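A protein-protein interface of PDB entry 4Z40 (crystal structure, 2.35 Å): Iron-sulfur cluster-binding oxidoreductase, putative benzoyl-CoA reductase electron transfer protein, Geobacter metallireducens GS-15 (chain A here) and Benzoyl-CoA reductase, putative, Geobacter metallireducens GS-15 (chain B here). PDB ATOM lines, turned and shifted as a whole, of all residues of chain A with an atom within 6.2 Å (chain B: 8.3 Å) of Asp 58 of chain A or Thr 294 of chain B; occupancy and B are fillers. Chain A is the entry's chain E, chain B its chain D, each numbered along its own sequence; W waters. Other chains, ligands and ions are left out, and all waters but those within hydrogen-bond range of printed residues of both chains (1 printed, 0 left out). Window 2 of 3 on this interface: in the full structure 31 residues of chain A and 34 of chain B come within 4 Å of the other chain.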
ATOM      1  N   ASP A  54     -21.165 -16.798  19.582  1.00  0.00           N
ATOM      2  CA  ASP A  54     -21.222 -18.256  19.656  1.00  0.00           C
ATOM      3  C   ASP A  54     -20.664 -18.706  21.002  1.00  0.00           C
ATOM      4  O   ASP A  54     -19.446 -18.746  21.197  1.00  0.00           O
ATOM      5  CB  ASP A  54     -20.455 -18.916  18.510  1.00  0.00           C
ATOM      6  CG  ASP A  54     -20.707 -20.423  18.423  1.00  0.00           C
ATOM      7  OD1 ASP A  54     -20.994 -21.061  19.466  1.00  0.00           O
ATOM      8  OD2 ASP A  54     -20.620 -20.977  17.307  1.00  0.00           O
ATOM      9  N   PRO A  55     -21.557 -19.044  21.938  1.00  0.00           N
ATOM     10  CA  PRO A  55     -21.173 -19.432  23.295  1.00  0.00           C
ATOM     11  C   PRO A  55     -20.373 -20.730  23.328  1.00  0.00           C
ATOM     12  O   PRO A  55     -19.488 -20.878  24.154  1.00  0.00           O
ATOM     13  CB  PRO A  55     -22.524 -19.603  24.002  1.00  0.00           C
ATOM     14  CG  PRO A  55     -23.515 -18.864  23.135  1.00  0.00           C
ATOM     15  CD  PRO A  55     -23.017 -19.059  21.754  1.00  0.00           C
ATOM     16  N   LEU A  56     -20.691 -21.659  22.435  1.00  0.00           N
ATOM     17  CA  LEU A  56     -19.990 -22.938  22.368  1.00  0.00           C
ATOM     18  C   LEU A  56     -18.541 -22.784  21.908  1.00  0.00           C
ATOM     19  O   LEU A  56     -17.688 -23.601  22.249  1.00  0.00           O
ATOM     20  CB  LEU A  56     -20.727 -23.883  21.426  1.00  0.00           C
ATOM     21  CG  LEU A  56     -22.182 -24.138  21.797  1.00  0.00           C
ATOM     22  CD1 LEU A  56     -22.925 -24.789  20.643  1.00  0.00           C
ATOM     23  CD2 LEU A  56     -22.241 -25.008  23.043  1.00  0.00           C
ATOM     24  N   ARG A  57     -18.277 -21.742  21.125  1.00  0.00           N
ATOM     25  CA  ARG A  57     -16.938 -21.465  20.617  1.00  0.00           C
ATOM     26  C   ARG A  57     -16.172 -20.446  21.472  1.00  0.00           C
ATOM     27  O   ARG A  57     -15.031 -20.100  21.149  1.00  0.00           O
ATOM     28  CB  ARG A  57     -17.014 -20.955  19.171  1.00  0.00           C
ATOM     29  CG  ARG A  57     -17.377 -22.012  18.123  1.00  0.00           C
ATOM     30  CD  ARG A  57     -17.278 -21.443  16.696  1.00  0.00           C
ATOM     31  NE  ARG A  57     -18.477 -20.694  16.325  1.00  0.00           N
ATOM     32  CZ  ARG A  57     -18.525 -19.750  15.387  1.00  0.00           C
ATOM     33  NH1 ARG A  57     -17.435 -19.413  14.704  1.00  0.00           N
ATOM     34  NH2 ARG A  57     -19.671 -19.132  15.133  1.00  0.00           N
ATOM     35  N   ASP A  58     -16.810 -19.977  22.547  1.00  0.00           N
ATOM     36  CA  ASP A  58     -16.297 -18.917  23.425  1.00  0.00           C
ATOM     37  C   ASP A  58     -16.097 -17.601  22.662  1.00  0.00           C
ATOM     38  O   ASP A  58     -15.181 -16.827  22.951  1.00  0.00           O
ATOM     39  CB  ASP A  58     -14.991 -19.350  24.102  1.00  0.00           C
ATOM     40  CG  ASP A  58     -14.569 -18.403  25.228  1.00  0.00           C
ATOM     41  OD1 ASP A  58     -15.464 -17.821  25.884  1.00  0.00           O
ATOM     42  OD2 ASP A  58     -13.348 -18.229  25.449  1.00  0.00           O
ATOM     43  N   ILE A  59     -16.963 -17.346  21.685  1.00  0.00           N
ATOM     44  CA  ILE A  59     -16.849 -16.145  20.868  1.00  0.00           C
ATOM     45  C   ILE A  59     -17.935 -15.136  21.225  1.00  0.00           C
ATOM     46  O   ILE A  59     -19.122 -15.437  21.155  1.00  0.00           O
ATOM     47  CB  ILE A  59     -16.929 -16.473  19.351  1.00  0.00           C
ATOM     48  CG1 ILE A  59     -15.774 -17.385  18.946  1.00  0.00           C
ATOM     49  CG2 ILE A  59     -16.922 -15.199  18.512  1.00  0.00           C
ATOM     50  CD1 ILE A  59     -15.748 -17.693  17.473  1.00  0.00           C
ATOM     51  N   TYR A  60     -17.506 -13.942  21.616  1.00  0.00           N
ATOM     52  CA  TYR A  60     -18.404 -12.834  21.925  1.00  0.00           C
ATOM     53  C   TYR A  60     -17.724 -11.567  21.457  1.00  0.00           C
ATOM     54  O   TYR A  60     -16.773 -11.098  22.089  1.00  0.00           O
ATOM     55  CB  TYR A  60     -18.718 -12.743  23.423  1.00  0.00           C
ATOM     56  CG  TYR A  60     -19.225 -14.029  24.028  1.00  0.00           C
ATOM     57  CD1 TYR A  60     -18.341 -15.010  24.443  1.00  0.00           C
ATOM     58  CD2 TYR A  60     -20.591 -14.258  24.190  1.00  0.00           C
ATOM     59  CE1 TYR A  60     -18.797 -16.185  24.985  1.00  0.00           C
ATOM     60  CE2 TYR A  60     -21.052 -15.418  24.726  1.00  0.00           C
ATOM     61  CZ  TYR A  60     -20.153 -16.384  25.133  1.00  0.00           C
ATOM     62  OH  TYR A  60     -20.596 -17.562  25.694  1.00  0.00           O
ATOM     63  N   LYS A  84      -9.646 -20.221  17.920  1.00  0.00           N
ATOM     64  CA  LYS A  84     -11.062 -19.979  17.649  1.00  0.00           C
ATOM     65  C   LYS A  84     -11.346 -19.851  16.163  1.00  0.00           C
ATOM     66  O   LYS A  84     -10.659 -19.131  15.451  1.00  0.00           O
ATOM     67  CB  LYS A  84     -11.535 -18.719  18.372  1.00  0.00           C
ATOM     68  CG  LYS A  84     -11.424 -18.797  19.872  1.00  0.00           C
ATOM     69  CD  LYS A  84     -11.859 -17.503  20.527  1.00  0.00           C
ATOM     70  CE  LYS A  84     -12.260 -17.757  21.979  1.00  0.00           C
ATOM     71  NZ  LYS A  84     -12.531 -16.492  22.707  1.00  0.00           N
ATOM     72  N   MET B 252     -21.946 -20.339  40.125  1.00  0.00           N
ATOM     73  CA  MET B 252     -20.864 -20.475  39.147  1.00  0.00           C
ATOM     74  C   MET B 252     -19.685 -19.553  39.488  1.00  0.00           C
ATOM     75  O   MET B 252     -18.546 -19.808  39.097  1.00  0.00           O
ATOM     76  CB  MET B 252     -21.378 -20.200  37.728  1.00  0.00           C
ATOM     77  CG  MET B 252     -22.541 -21.078  37.323  1.00  0.00           C
ATOM     78  SD  MET B 252     -22.345 -22.794  37.858  1.00  0.00           S
ATOM     79  CE  MET B 252     -21.289 -23.429  36.572  1.00  0.00           C
ATOM     80  N   MET B 289     -12.877 -26.234  39.150  1.00  0.00           N
ATOM     81  CA  MET B 289     -13.776 -25.189  38.675  1.00  0.00           C
ATOM     82  C   MET B 289     -13.047 -24.106  37.884  1.00  0.00           C
ATOM     83  O   MET B 289     -13.575 -23.593  36.903  1.00  0.00           O
ATOM     84  CB  MET B 289     -14.516 -24.566  39.863  1.00  0.00           C
ATOM     85  CG  MET B 289     -15.734 -23.747  39.496  1.00  0.00           C
ATOM     86  SD  MET B 289     -17.078 -24.751  38.832  1.00  0.00           S
ATOM     87  CE  MET B 289     -18.175 -23.459  38.247  1.00  0.00           C
ATOM     88  N   ASP B 290     -11.835 -23.760  38.312  1.00  0.00           N
ATOM     89  CA  ASP B 290     -11.028 -22.774  37.598  1.00  0.00           C
ATOM     90  C   ASP B 290     -10.666 -23.288  36.213  1.00  0.00           C
ATOM     91  O   ASP B 290     -10.537 -22.516  35.259  1.00  0.00           O
ATOM     92  CB  ASP B 290      -9.749 -22.438  38.373  1.00  0.00           C
ATOM     93  CG  ASP B 290     -10.025 -21.672  39.657  1.00  0.00           C
ATOM     94  OD1 ASP B 290     -11.171 -21.208  39.841  1.00  0.00           O
ATOM     95  OD2 ASP B 290      -9.092 -21.531  40.483  1.00  0.00           O
ATOM     96  N   LYS B 291     -10.503 -24.602  36.117  1.00  0.00           N
ATOM     97  CA  LYS B 291     -10.110 -25.250  34.879  1.00  0.00           C
ATOM     98  C   LYS B 291     -11.297 -25.411  33.925  1.00  0.00           C
ATOM     99  O   LYS B 291     -11.141 -25.334  32.703  1.00  0.00           O
ATOM    100  CB  LYS B 291      -9.483 -26.611  35.190  1.00  0.00           C
ATOM    101  CG  LYS B 291      -8.848 -27.325  34.005  1.00  0.00           C
ATOM    102  CD  LYS B 291      -8.372 -28.718  34.409  1.00  0.00           C
ATOM    103  CE  LYS B 291      -7.427 -28.661  35.601  1.00  0.00           C
ATOM    104  NZ  LYS B 291      -7.054 -30.019  36.096  1.00  0.00           N
ATOM    105  N   ALA B 292     -12.484 -25.615  34.486  1.00  0.00           N
ATOM    106  CA  ALA B 292     -13.658 -25.955  33.686  1.00  0.00           C
ATOM    107  C   ALA B 292     -14.496 -24.747  33.294  1.00  0.00           C
ATOM    108  O   ALA B 292     -15.168 -24.769  32.262  1.00  0.00           O
ATOM    109  CB  ALA B 292     -14.524 -26.954  34.432  1.00  0.00           C
ATOM    110  N   ARG B 293     -14.476 -23.701  34.115  1.00  0.00           N
ATOM    111  CA  ARG B 293     -15.292 -22.522  33.832  1.00  0.00           C
ATOM    112  C   ARG B 293     -14.628 -21.668  32.753  1.00  0.00           C
ATOM    113  O   ARG B 293     -13.554 -21.114  32.949  1.00  0.00           O
ATOM    114  CB  ARG B 293     -15.533 -21.698  35.099  1.00  0.00           C
ATOM    115  CG  ARG B 293     -16.533 -20.561  34.912  1.00  0.00           C
ATOM    116  CD  ARG B 293     -16.718 -19.747  36.189  1.00  0.00           C
ATOM    117  NE  ARG B 293     -15.443 -19.467  36.848  1.00  0.00           N
ATOM    118  CZ  ARG B 293     -15.127 -19.891  38.069  1.00  0.00           C
ATOM    119  NH1 ARG B 293     -16.001 -20.600  38.774  1.00  0.00           N
ATOM    120  NH2 ARG B 293     -13.944 -19.597  38.594  1.00  0.00           N
ATOM    121  N   THR B 294     -15.283 -21.579  31.606  1.00  0.00           N
ATOM    122  CA  THR B 294     -14.746 -20.870  30.459  1.00  0.00           C
ATOM    123  C   THR B 294     -15.136 -19.400  30.493  1.00  0.00           C
ATOM    124  O   THR B 294     -14.296 -18.538  30.327  1.00  0.00           O
ATOM    125  CB  THR B 294     -15.239 -21.501  29.159  1.00  0.00           C
ATOM    126  OG1 THR B 294     -14.866 -22.884  29.137  1.00  0.00           O
ATOM    127  CG2 THR B 294     -14.642 -20.780  27.951  1.00  0.00           C
ATOM    128  N   ARG B 295     -16.418 -19.117  30.710  1.00  0.00           N
ATOM    129  CA  ARG B 295     -16.871 -17.732  30.799  1.00  0.00           C
ATOM    130  C   ARG B 295     -18.202 -17.630  31.531  1.00  0.00           C
ATOM    131  O   ARG B 295     -19.031 -18.516  31.438  1.00  0.00           O
ATOM    132  CB  ARG B 295     -16.999 -17.106  29.403  1.00  0.00           C
ATOM    133  CG  ARG B 295     -17.205 -15.594  29.423  1.00  0.00           C
ATOM    134  CD  ARG B 295     -17.447 -15.025  28.034  1.00  0.00           C
ATOM    135  NE  ARG B 295     -16.293 -15.237  27.159  1.00  0.00           N
ATOM    136  CZ  ARG B 295     -15.723 -14.293  26.421  1.00  0.00           C
ATOM    137  NH1 ARG B 295     -16.195 -13.051  26.433  1.00  0.00           N
ATOM    138  NH2 ARG B 295     -14.673 -14.597  25.674  1.00  0.00           N
ATOM    139  N   LEU B 296     -18.381 -16.542  32.267  1.00  0.00           N
ATOM    140  CA  LEU B 296     -19.654 -16.221  32.887  1.00  0.00           C
ATOM    141  C   LEU B 296     -20.482 -15.434  31.891  1.00  0.00           C
ATOM    142  O   LEU B 296     -20.044 -14.403  31.415  1.00  0.00           O
ATOM    143  CB  LEU B 296     -19.446 -15.418  34.174  1.00  0.00           C
ATOM    144  CG  LEU B 296     -18.665 -16.129  35.280  1.00  0.00           C
ATOM    145  CD1 LEU B 296     -18.123 -15.119  36.302  1.00  0.00           C
ATOM    146  CD2 LEU B 296     -19.558 -17.193  35.961  1.00  0.00           C
ATOM    147  N   ILE B 297     -21.674 -15.923  31.568  1.00  0.00           N
ATOM    148  CA  ILE B 297     -22.479 -15.322  30.501  1.00  0.00           C
ATOM    149  C   ILE B 297     -23.904 -15.016  30.956  1.00  0.00           C
ATOM    150  O   ILE B 297     -24.430 -15.665  31.860  1.00  0.00           O
ATOM    151  CB  ILE B 297     -22.531 -16.239  29.261  1.00  0.00           C
ATOM    152  CG1 ILE B 297     -23.168 -17.588  29.607  1.00  0.00           C
ATOM    153  CG2 ILE B 297     -21.140 -16.448  28.701  1.00  0.00           C
ATOM    154  CD1 ILE B 297     -23.429 -18.456  28.392  1.00  0.00           C
ATOM    155  N   GLY B 307     -24.951 -17.565  34.505  1.00  0.00           N
ATOM    156  CA  GLY B 307     -24.564 -18.823  33.891  1.00  0.00           C
ATOM    157  C   GLY B 307     -23.081 -18.923  33.621  1.00  0.00           C
ATOM    158  O   GLY B 307     -22.364 -17.931  33.658  1.00  0.00           O
ATOM    159  N   ALA B 308     -22.617 -20.131  33.346  1.00  0.00           N
ATOM    160  CA  ALA B 308     -21.240 -20.330  32.935  1.00  0.00           C
ATOM    161  C   ALA B 308     -21.113 -21.455  31.912  1.00  0.00           C
ATOM    162  O   ALA B 308     -21.711 -22.530  32.071  1.00  0.00           O
ATOM    163  CB  ALA B 308     -20.378 -20.621  34.132  1.00  0.00           C
ATOM    164  N   THR B 309     -20.330 -21.208  30.867  1.00  0.00           N
ATOM    165  CA  THR B 309     -19.955 -22.266  29.940  1.00  0.00           C
ATOM    166  C   THR B 309     -18.960 -23.201  30.620  1.00  0.00           C
ATOM    167  O   THR B 309     -18.024 -22.755  31.277  1.00  0.00           O
ATOM    168  CB  THR B 309     -19.340 -21.710  28.637  1.00  0.00           C
ATOM    169  OG1 THR B 309     -18.369 -20.714  28.962  1.00  0.00           O
ATOM    170  CG2 THR B 309     -20.410 -21.086  27.764  1.00  0.00           C
ATOM    171  N   ILE B 310     -19.180 -24.500  30.472  1.00  0.00           N
ATOM    172  CA  ILE B 310     -18.340 -25.490  31.128  1.00  0.00           C
ATOM    173  C   ILE B 310     -17.648 -26.372  30.112  1.00  0.00           C
ATOM    174  O   ILE B 310     -18.295 -26.957  29.236  1.00  0.00           O
ATOM    175  CB  ILE B 310     -19.155 -26.379  32.086  1.00  0.00           C
ATOM    176  CG1 ILE B 310     -19.797 -25.517  33.182  1.00  0.00           C
ATOM    177  CG2 ILE B 310     -18.268 -27.473  32.683  1.00  0.00           C
ATOM    178  CD1 ILE B 310     -18.817 -24.842  34.101  1.00  0.00           C
ATOM    179  N   SER B 311     -16.332 -26.480  30.236  1.00  0.00           N
ATOM    180  CA  SER B 311     -15.575 -27.292  29.307  1.00  0.00           C
ATOM    181  C   SER B 311     -14.699 -28.313  30.024  1.00  0.00           C
ATOM    182  O   SER B 311     -13.621 -27.986  30.515  1.00  0.00           O
ATOM    183  CB  SER B 311     -14.725 -26.400  28.405  1.00  0.00           C
ATOM    184  OG  SER B 311     -14.082 -27.188  27.427  1.00  0.00           O
ATOM    185  N   MET B 312     -15.177 -29.551  30.086  1.00  0.00           N
ATOM    186  CA  MET B 312     -14.397 -30.657  30.632  1.00  0.00           C
ATOM    187  C   MET B 312     -13.591 -31.306  29.518  1.00  0.00           C
ATOM    188  O   MET B 312     -14.023 -31.323  28.368  1.00  0.00           O
ATOM    189  CB  MET B 312     -15.300 -31.696  31.299  1.00  0.00           C
ATOM    190  CG  MET B 312     -16.233 -31.118  32.343  1.00  0.00           C
ATOM    191  SD  MET B 312     -15.317 -30.346  33.697  1.00  0.00           S
ATOM    192  CE  MET B 312     -14.551 -31.781  34.457  1.00  0.00           C
ATOM    193  N   THR B 317     -18.755 -28.626  25.042  1.00  0.00           N
ATOM    194  CA  THR B 317     -19.076 -27.563  25.968  1.00  0.00           C
ATOM    195  C   THR B 317     -20.571 -27.521  26.239  1.00  0.00           C
ATOM    196  O   THR B 317     -21.378 -27.797  25.354  1.00  0.00           O
ATOM    197  CB  THR B 317     -18.595 -26.213  25.415  1.00  0.00           C
ATOM    198  OG1 THR B 317     -17.167 -26.247  25.296  1.00  0.00           O
ATOM    199  CG2 THR B 317     -18.994 -25.057  26.321  1.00  0.00           C
ATOM    200  N   TYR B 318     -20.942 -27.207  27.476  1.00  0.00           N
ATOM    201  CA  TYR B 318     -22.342 -26.954  27.799  1.00  0.00           C
ATOM    202  C   TYR B 318     -22.435 -25.768  28.761  1.00  0.00           C
ATOM    203  O   TYR B 318     -21.411 -25.202  29.141  1.00  0.00           O
ATOM    204  CB  TYR B 318     -23.002 -28.204  28.381  1.00  0.00           C
ATOM    205  CG  TYR B 318     -22.542 -28.581  29.772  1.00  0.00           C
ATOM    206  CD1 TYR B 318     -21.283 -29.133  29.984  1.00  0.00           C
ATOM    207  CD2 TYR B 318     -23.381 -28.409  30.871  1.00  0.00           C
ATOM    208  CE1 TYR B 318     -20.864 -29.491  31.248  1.00  0.00           C
ATOM    209  CE2 TYR B 318     -22.976 -28.767  32.139  1.00  0.00           C
ATOM    210  CZ  TYR B 318     -21.716 -29.309  32.323  1.00  0.00           C
ATOM    211  OH  TYR B 318     -21.309 -29.661  33.591  1.00  0.00           O
HETATM  212  O   HOH W   1     -18.154 -19.144  26.447  1.00  0.00           O
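The side-chain carboxylate (OD1) of Asp 58 of chain A lies within salt-bridge range of the guanidinium group (NE) of Arg 295 of chain B (3.0 Å).
The backbone NH of Thr 294 of chain B sits at hydrogen-bond distance from the backbone carbonyl oxygen of Thr 309 of chain B.
N of Thr 309 of chain B lies within hydrogen-bond range of O of Arg 295 of chain B (3.0 Å).
The backbone NH (N) of Ile 297 of chain B is in hydrogen-bond range of the backbone carbonyl oxygen (O) of Gly 307 of chain B, 3.0 Å away.
The side-chain carboxylate (OD1) of Asp 54 of chain A is in hydrogen-bond range of the backbone NH (N) of Leu 56 of chain A (3.0 Å).
OD2 of Asp 58 of chain A is in salt-bridge range of NZ of Lys 84 of chain A (3.3 Å).
Thr 309 of chain B touches Pro 55 of chain A.
CD2 of Leu 56 of chain A touches O of Thr 317 of chain B, 3.7 Å away.
CG of Asp 58 of chain A touches CG2 of Thr 294 of chain B, at 3.6 Å.
Tyr 60 of chain A touches Arg 295 of chain B (CD1 to CZ, 3.4 Å).
Tyr 60 of chain A touches Ile 297 of chain B.
Asp 58 of chain A touches two residues of chain B.
Of chain A, only Asp 58 (3.6 Å) comes within 4 Å of Thr 294 of chain B.
Printed residues of chain B within 4 Å of Leu 56 of chain A: Thr 317 (3.7 Å).
Of the printed residues of chain A, Ile 297 of chain B touches Tyr 60.
Printed residues of chain B within 4 Å of Pro 55 of chain A: Thr 309.
Ile 310 of chain B touches none of the printed residues of chain A.
Met 252 of chain B touches none of the printed residues of chain A.
The nearest residue of chain B that does not touch Asp 58 of chain A is Thr 309 of chain B (5.1 Å).
Hydrophobic or aromatic side chains of chain A that line the printed part of chain B: Leu 56 and Tyr 60.
Of the 18 printed residues of chain B, 5 touch a printed residue of chain A.
Hydrophobic or aromatic side chains of chain B within 4 Å of the printed part of chain A: Ile 297.
Among the printed residues, Asp or Glu carboxylates within 4 Å of a Lys or Arg side-chain nitrogen of the other chain: Asp 58 of chain A with Arg 295 of chain B (3.0 Å).
Water W1 lies within hydrogen-bond range of the side-chain hydroxyl (OG1) of Thr 309 of chain B (3.0 Å), the side-chain hydroxyl (OH) of Tyr 60 of chain A (3.0 Å), the side-chain carboxylate (OD1) of Asp 58 of chain A (3.1 Å) and the backbone carbonyl oxygen (O) of Pro 55 of chain A (3.2 Å).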
